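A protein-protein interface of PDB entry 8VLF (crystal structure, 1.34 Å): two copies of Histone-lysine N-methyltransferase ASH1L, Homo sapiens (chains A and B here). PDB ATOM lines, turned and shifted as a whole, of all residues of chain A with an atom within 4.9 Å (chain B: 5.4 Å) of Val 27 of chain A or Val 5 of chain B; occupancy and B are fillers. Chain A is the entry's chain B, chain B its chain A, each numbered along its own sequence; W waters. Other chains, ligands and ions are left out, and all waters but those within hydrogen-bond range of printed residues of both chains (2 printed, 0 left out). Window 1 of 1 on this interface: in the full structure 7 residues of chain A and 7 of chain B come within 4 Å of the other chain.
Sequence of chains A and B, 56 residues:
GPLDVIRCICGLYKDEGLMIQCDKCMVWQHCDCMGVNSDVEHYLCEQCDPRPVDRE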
ATOM      1  N   VAL A   5       8.708 -26.026  17.760  1.00  0.00           N
ATOM      2  CA  VAL A   5      10.073 -25.508  17.689  1.00  0.00           C
ATOM      3  C   VAL A   5      10.839 -26.023  18.899  1.00  0.00           C
ATOM      4  O   VAL A   5      10.421 -25.816  20.043  1.00  0.00           O
ATOM      5  CB  VAL A   5      10.108 -23.972  17.642  1.00  0.00           C
ATOM      6  CG1 VAL A   5      11.562 -23.485  17.658  1.00  0.00           C
ATOM      7  CG2 VAL A   5       9.385 -23.452  16.388  1.00  0.00           C
ATOM      8  N   ARG A   7      14.131 -25.399  20.928  1.00  0.00           N
ATOM      9  CA  ARG A   7      15.230 -24.445  21.107  1.00  0.00           C
ATOM     10  C   ARG A   7      15.716 -24.587  22.543  1.00  0.00           C
ATOM     11  O   ARG A   7      15.265 -23.863  23.431  1.00  0.00           O
ATOM     12  CB  ARG A   7      14.842 -23.006  20.801  1.00  0.00           C
ATOM     13  CG  ARG A   7      16.087 -22.131  20.718  1.00  0.00           C
ATOM     14  CD  ARG A   7      15.824 -20.654  20.922  1.00  0.00           C
ATOM     15  NE  ARG A   7      15.249 -20.367  22.232  1.00  0.00           N
ATOM     16  CZ  ARG A   7      15.912 -20.409  23.394  1.00  0.00           C
ATOM     17  NH1 ARG A   7      17.195 -20.750  23.439  1.00  0.00           N
ATOM     18  NH2 ARG A   7      15.280 -20.119  24.532  1.00  0.00           N
ATOM     19  N   ILE A  20       9.909 -29.764  27.880  1.00  0.00           N
ATOM     20  CA  ILE A  20       9.015 -28.801  28.512  1.00  0.00           C
ATOM     21  C   ILE A  20       8.911 -27.578  27.612  1.00  0.00           C
ATOM     22  O   ILE A  20       9.889 -27.193  26.962  1.00  0.00           O
ATOM     23  CB  ILE A  20       9.508 -28.441  29.940  1.00  0.00           C
ATOM     24  CG1 ILE A  20       8.468 -27.611  30.707  1.00  0.00           C
ATOM     25  CG2 ILE A  20      10.888 -27.779  29.904  1.00  0.00           C
ATOM     26  CD1 ILE A  20       8.707 -27.612  32.227  1.00  0.00           C
ATOM     27  N   GLN A  21       7.727 -26.985  27.558  1.00  0.00           N
ATOM     28  CA  GLN A  21       7.449 -25.870  26.665  1.00  0.00           C
ATOM     29  C   GLN A  21       7.470 -24.552  27.429  1.00  0.00           C
ATOM     30  O   GLN A  21       6.914 -24.447  28.528  1.00  0.00           O
ATOM     31  CB  GLN A  21       6.082 -26.041  26.009  1.00  0.00           C
ATOM     32  CG  GLN A  21       5.730 -24.918  25.038  1.00  0.00           C
ATOM     33  CD  GLN A  21       4.493 -25.232  24.225  1.00  0.00           C
ATOM     34  OE1 GLN A  21       3.436 -25.555  24.776  1.00  0.00           O
ATOM     35  NE2 GLN A  21       4.607 -25.126  22.912  1.00  0.00           N
ATOM     36  N   CYS A  22       8.116 -23.544  26.847  1.00  0.00           N
ATOM     37  CA  CYS A  22       8.084 -22.209  27.431  1.00  0.00           C
ATOM     38  C   CYS A  22       6.673 -21.641  27.332  1.00  0.00           C
ATOM     39  O   CYS A  22       6.052 -21.664  26.260  1.00  0.00           O
ATOM     40  CB  CYS A  22       9.072 -21.280  26.716  1.00  0.00           C
ATOM     41  SG  CYS A  22       9.073 -19.568  27.361  1.00  0.00           S
ATOM     42  N   CYS A  25       7.107 -18.015  24.747  1.00  0.00           N
ATOM     43  CA  CYS A  25       7.552 -18.096  23.355  1.00  0.00           C
ATOM     44  C   CYS A  25       7.281 -19.447  22.703  1.00  0.00           C
ATOM     45  O   CYS A  25       7.488 -19.586  21.492  1.00  0.00           O
ATOM     46  CB  CYS A  25       9.040 -17.738  23.232  1.00  0.00           C
ATOM     47  SG  CYS A  25      10.172 -19.000  23.846  1.00  0.00           S
ATOM     48  N   MET A  26       6.852 -20.452  23.470  1.00  0.00           N
ATOM     49  CA  MET A  26       6.397 -21.759  22.977  1.00  0.00           C
ATOM     50  C   MET A  26       7.499 -22.707  22.514  1.00  0.00           C
ATOM     51  O   MET A  26       7.171 -23.781  22.004  1.00  0.00           O
ATOM     52  CB  MET A  26       5.272 -21.673  21.934  1.00  0.00           C
ATOM     53  CG  MET A  26       4.209 -20.648  22.313  1.00  0.00           C
ATOM     54  SD  MET A  26       3.331 -21.148  23.809  1.00  0.00           S
ATOM     55  CE  MET A  26       2.476 -22.608  23.234  1.00  0.00           C
ATOM     56  N   VAL A  27       8.783 -22.366  22.670  1.00  0.00           N
ATOM     57  CA  VAL A  27       9.828 -23.328  22.328  1.00  0.00           C
ATOM     58  C   VAL A  27       9.843 -24.481  23.323  1.00  0.00           C
ATOM     59  O   VAL A  27       9.415 -24.358  24.472  1.00  0.00           O
ATOM     60  CB  VAL A  27      11.221 -22.689  22.208  1.00  0.00           C
ATOM     61  CG1 VAL A  27      11.196 -21.538  21.221  1.00  0.00           C
ATOM     62  CG2 VAL A  27      11.780 -22.275  23.575  1.00  0.00           C
ATOM     63  N   TRP A  28      10.353 -25.619  22.867  1.00  0.00           N
ATOM     64  CA  TRP A  28      10.522 -26.806  23.690  1.00  0.00           C
ATOM     65  C   TRP A  28      11.988 -26.975  24.063  1.00  0.00           C
ATOM     66  O   TRP A  28      12.891 -26.765  23.240  1.00  0.00           O
ATOM     67  CB  TRP A  28      10.048 -28.041  22.922  1.00  0.00           C
ATOM     68  CG  TRP A  28       8.573 -28.073  22.710  1.00  0.00           C
ATOM     69  CD1 TRP A  28       7.875 -27.532  21.664  1.00  0.00           C
ATOM     70  CD2 TRP A  28       7.595 -28.671  23.574  1.00  0.00           C
ATOM     71  NE1 TRP A  28       6.538 -27.763  21.822  1.00  0.00           N
ATOM     72  CE2 TRP A  28       6.336 -28.453  22.989  1.00  0.00           C
ATOM     73  CE3 TRP A  28       7.666 -29.367  24.793  1.00  0.00           C
ATOM     74  CZ2 TRP A  28       5.154 -28.912  23.574  1.00  0.00           C
ATOM     75  CZ3 TRP A  28       6.499 -29.815  25.367  1.00  0.00           C
ATOM     76  CH2 TRP A  28       5.259 -29.589  24.761  1.00  0.00           C
ATOM     77  N   GLN A  29      12.219 -27.361  25.306  1.00  0.00           N
ATOM     78  CA  GLN A  29      13.555 -27.544  25.841  1.00  0.00           C
ATOM     79  C   GLN A  29      13.624 -28.885  26.561  1.00  0.00           C
ATOM     80  O   GLN A  29      12.607 -29.411  27.026  1.00  0.00           O
ATOM     81  CB  GLN A  29      13.921 -26.387  26.786  1.00  0.00           C
ATOM     82  CG  GLN A  29      13.656 -25.000  26.184  1.00  0.00           C
ATOM     83  CD  GLN A  29      14.411 -23.895  26.897  1.00  0.00           C
ATOM     84  OE1 GLN A  29      14.175 -23.644  28.076  1.00  0.00           O
ATOM     85  NE2 GLN A  29      15.325 -23.226  26.198  1.00  0.00           N
ATOM     86  N   CYS A  45      11.631 -20.213  29.323  1.00  0.00           N
ATOM     87  CA  CYS A  45      12.967 -20.501  28.843  1.00  0.00           C
ATOM     88  C   CYS A  45      13.966 -19.447  29.331  1.00  0.00           C
ATOM     89  O   CYS A  45      13.604 -18.444  29.957  1.00  0.00           O
ATOM     90  CB  CYS A  45      12.948 -20.614  27.320  1.00  0.00           C
ATOM     91  SG  CYS A  45      12.833 -19.015  26.466  1.00  0.00           S
ATOM     92  N   GLY B   1      11.837  -9.180  19.402  1.00  0.00           N
ATOM     93  CA  GLY B   1      11.575  -9.028  20.823  1.00  0.00           C
ATOM     94  C   GLY B   1      11.256 -10.336  21.521  1.00  0.00           C
ATOM     95  O   GLY B   1      11.407 -11.395  20.932  1.00  0.00           O
ATOM     96  N   LEU B   3       8.674 -12.078  22.170  1.00  0.00           N
ATOM     97  CA  LEU B   3       7.727 -12.987  21.540  1.00  0.00           C
ATOM     98  C   LEU B   3       8.265 -13.592  20.251  1.00  0.00           C
ATOM     99  O   LEU B   3       7.673 -14.550  19.742  1.00  0.00           O
ATOM    100  CB  LEU B   3       6.437 -12.226  21.233  1.00  0.00           C
ATOM    101  CG  LEU B   3       5.751 -11.619  22.456  1.00  0.00           C
ATOM    102  CD1 LEU B   3       4.704 -10.582  22.058  1.00  0.00           C
ATOM    103  CD2 LEU B   3       5.136 -12.728  23.285  1.00  0.00           C
ATOM    104  N   ASP B   4       9.353 -13.051  19.707  1.00  0.00           N
ATOM    105  CA  ASP B   4       9.949 -13.571  18.486  1.00  0.00           C
ATOM    106  C   ASP B   4      11.023 -14.570  18.875  1.00  0.00           C
ATOM    107  O   ASP B   4      11.788 -14.334  19.814  1.00  0.00           O
ATOM    108  CB  ASP B   4      10.593 -12.442  17.683  1.00  0.00           C
ATOM    109  CG  ASP B   4       9.624 -11.319  17.380  1.00  0.00           C
ATOM    110  OD1 ASP B   4       8.459 -11.612  17.045  1.00  0.00           O
ATOM    111  OD2 ASP B   4      10.034 -10.140  17.468  1.00  0.00           O
ATOM    112  N   VAL B   5      11.076 -15.690  18.165  1.00  0.00           N
ATOM    113  CA  VAL B   5      12.036 -16.751  18.465  1.00  0.00           C
ATOM    114  C   VAL B   5      13.150 -16.675  17.437  1.00  0.00           C
ATOM    115  O   VAL B   5      12.893 -16.731  16.232  1.00  0.00           O
ATOM    116  CB  VAL B   5      11.390 -18.146  18.452  1.00  0.00           C
ATOM    117  CG1 VAL B   5      12.458 -19.218  18.690  1.00  0.00           C
ATOM    118  CG2 VAL B   5      10.294 -18.243  19.521  1.00  0.00           C
ATOM    119  N   ILE B   6      14.383 -16.545  17.907  1.00  0.00           N
ATOM    120  CA  ILE B   6      15.564 -16.640  17.059  1.00  0.00           C
ATOM    121  C   ILE B   6      16.062 -18.077  17.142  1.00  0.00           C
ATOM    122  O   ILE B   6      16.351 -18.579  18.233  1.00  0.00           O
ATOM    123  CB  ILE B   6      16.653 -15.645  17.497  1.00  0.00           C
ATOM    124  CG1 ILE B   6      16.150 -14.204  17.341  1.00  0.00           C
ATOM    125  CG2 ILE B   6      17.928 -15.860  16.683  1.00  0.00           C
ATOM    126  CD1 ILE B   6      17.128 -13.153  17.813  1.00  0.00           C
ATOM    127  N   ARG B   7      16.151 -18.760  16.006  1.00  0.00           N
ATOM    128  CA  ARG B   7      16.735 -20.108  15.995  1.00  0.00           C
ATOM    129  C   ARG B   7      17.484 -20.261  14.680  1.00  0.00           C
ATOM    130  O   ARG B   7      16.928 -20.753  13.700  1.00  0.00           O
ATOM    131  CB  ARG B   7      15.712 -21.218  16.166  1.00  0.00           C
ATOM    132  CG  ARG B   7      16.412 -22.546  16.441  1.00  0.00           C
ATOM    133  CD  ARG B   7      15.563 -23.758  16.126  1.00  0.00           C
ATOM    134  NE  ARG B   7      15.175 -23.818  14.720  1.00  0.00           N
ATOM    135  CZ  ARG B   7      15.989 -24.132  13.707  1.00  0.00           C
ATOM    136  NH1 ARG B   7      17.275 -24.399  13.922  1.00  0.00           N
ATOM    137  NH2 ARG B   7      15.517 -24.164  12.459  1.00  0.00           N
ATOM    138  N   TYR B  13      21.773 -16.575  20.006  1.00  0.00           N
ATOM    139  CA  TYR B  13      20.500 -15.888  20.204  1.00  0.00           C
ATOM    140  C   TYR B  13      20.771 -14.394  20.153  1.00  0.00           C
ATOM    141  O   TYR B  13      20.807 -13.695  21.161  1.00  0.00           O
ATOM    142  CB  TYR B  13      19.836 -16.312  21.518  1.00  0.00           C
ATOM    143  CG  TYR B  13      18.336 -16.132  21.445  1.00  0.00           C
ATOM    144  CD1 TYR B  13      17.753 -14.872  21.573  1.00  0.00           C
ATOM    145  CD2 TYR B  13      17.504 -17.218  21.182  1.00  0.00           C
ATOM    146  CE1 TYR B  13      16.381 -14.714  21.474  1.00  0.00           C
ATOM    147  CE2 TYR B  13      16.126 -17.070  21.088  1.00  0.00           C
ATOM    148  CZ  TYR B  13      15.575 -15.815  21.217  1.00  0.00           C
ATOM    149  OH  TYR B  13      14.216 -15.672  21.101  1.00  0.00           O
ATOM    150  N   MET B  26       8.055 -20.135  11.999  1.00  0.00           N
ATOM    151  CA  MET B  26       8.132 -18.739  12.445  1.00  0.00           C
ATOM    152  C   MET B  26       9.419 -18.341  13.154  1.00  0.00           C
ATOM    153  O   MET B  26       9.506 -17.202  13.632  1.00  0.00           O
ATOM    154  CB  MET B  26       6.895 -18.250  13.214  1.00  0.00           C
ATOM    155  CG  MET B  26       5.610 -18.786  12.614  1.00  0.00           C
ATOM    156  SD  MET B  26       5.283 -17.956  11.044  1.00  0.00           S
ATOM    157  CE  MET B  26       5.034 -16.268  11.576  1.00  0.00           C
ATOM    158  N   VAL B  27      10.422 -19.218  13.238  1.00  0.00           N
ATOM    159  CA  VAL B  27      11.699 -18.788  13.792  1.00  0.00           C
ATOM    160  C   VAL B  27      12.387 -17.799  12.857  1.00  0.00           C
ATOM    161  O   VAL B  27      12.144 -17.755  11.645  1.00  0.00           O
ATOM    162  CB  VAL B  27      12.627 -19.963  14.133  1.00  0.00           C
ATOM    163  CG1 VAL B  27      11.920 -20.938  15.027  1.00  0.00           C
ATOM    164  CG2 VAL B  27      13.175 -20.631  12.874  1.00  0.00           C
ATOM    165  N   TRP B  28      13.263 -16.993  13.439  1.00  0.00           N
ATOM    166  CA  TRP B  28      14.080 -16.042  12.702  1.00  0.00           C
ATOM    167  C   TRP B  28      15.511 -16.552  12.607  1.00  0.00           C
ATOM    168  O   TRP B  28      16.063 -17.101  13.573  1.00  0.00           O
ATOM    169  CB  TRP B  28      14.066 -14.690  13.414  1.00  0.00           C
ATOM    170  CG  TRP B  28      12.738 -14.014  13.363  1.00  0.00           C
ATOM    171  CD1 TRP B  28      11.700 -14.161  14.245  1.00  0.00           C
ATOM    172  CD2 TRP B  28      12.284 -13.088  12.364  1.00  0.00           C
ATOM    173  NE1 TRP B  28      10.643 -13.380  13.863  1.00  0.00           N
ATOM    174  CE2 TRP B  28      10.973 -12.715  12.710  1.00  0.00           C
ATOM    175  CE3 TRP B  28      12.862 -12.541  11.204  1.00  0.00           C
ATOM    176  CZ2 TRP B  28      10.230 -11.817  11.942  1.00  0.00           C
ATOM    177  CZ3 TRP B  28      12.123 -11.657  10.449  1.00  0.00           C
ATOM    178  CH2 TRP B  28      10.824 -11.298  10.820  1.00  0.00           C
HETATM  179  O   HOH W   1       6.565 -17.464  19.859  1.00  0.00           O
HETATM  180  O   HOH W   2      13.094 -18.579  22.481  1.00  0.00           O
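CG1 of Val 5 of chain A touches CG1 of Val 27 of chain B, 3.7 Å away. Ile 6 of chain B touches Arg 7 of chain A (O to CD, 3.4 Å). NE of Arg 7 of chain A touches CE2 of Tyr 13 of chain B (3.6 Å). O of Cys 25 of chain A touches CG2 of Val 5 of chain B, at 3.7 Å. Val 5 of chain B touches Val 27 of chain A (CG1 to CG1, 3.7 Å).
Of the printed residues of chain B, Val 5 of chain A touches Val 27. Of the printed residues of chain B, Arg 7 of chain A touches Ile 6 (3.4 Å) and Tyr 13 (3.6 Å). Of chain B, only Val 5 comes within 4 Å of Val 27 of chain A. Val 5 of chain B touches just these residues of chain A: Cys 25 and Val 27. Printed residues of chain A within 4 Å of Ile 6 of chain B: Arg 7. Of the printed residues of chain A, Val 27 of chain B touches Val 5 (3.7 Å).
The backbone carbonyl oxygen of Asp 4 of chain B is in hydrogen-bond range of the side-chain hydroxyl of Tyr 13 of chain B, at 3.1 Å. N of Trp 28 of chain B sits at hydrogen-bond distance from O of Val 5 of chain B, 2.8 Å away. The side-chain hydroxyl (OH) of Tyr 13 of chain B sits at hydrogen-bond distance from the backbone NH (N) of Ile 6 of chain B. The backbone carbonyl oxygen (O) of Val 5 of chain A lies within hydrogen-bond range of the backbone NH (N) of Trp 28 of chain A. The side-chain sulfur of Cys 45 of chain A lies close to the guanidinium group of Arg 7 of chain A, 3.3 Å away. The backbone carbonyl oxygen (O) of Val 27 of chain A lies within hydrogen-bond range of the backbone NH (N) of Cys 22 of chain A (2.8 Å).
Val 5 of chain A touches Val 27 of chain B, and with the chains exchanged Val 27 of chain A touches Val 5 of chain B. 5 positions are printed for both chains. Of the 5 pairs that touch across the chains among the printed residues, 2 have their exchanged pair printed and touching as well.
Of the 10 printed residues of chain B, 4 touch a printed residue of chain A. Of the 11 printed residues of chain A, 4 touch a printed residue of chain B. Printed residues of chain A that touch a printed residue of chain B: Val 5, Arg 7, Cys 25 and Val 27. Among the printed residues, no Asp or Glu carboxylate lies within 4 Å of a Lys or Arg side-chain nitrogen of the other chain.
Water W2 lies within hydrogen-bond range of NE of Arg 7 of chain A (2.8 Å) and OH of Tyr 13 of chain B (3.4 Å). Water W1 bridges the backbone carbonyl oxygen of Cys 25 of chain A and the backbone carbonyl oxygen of Leu 3 of chain B.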
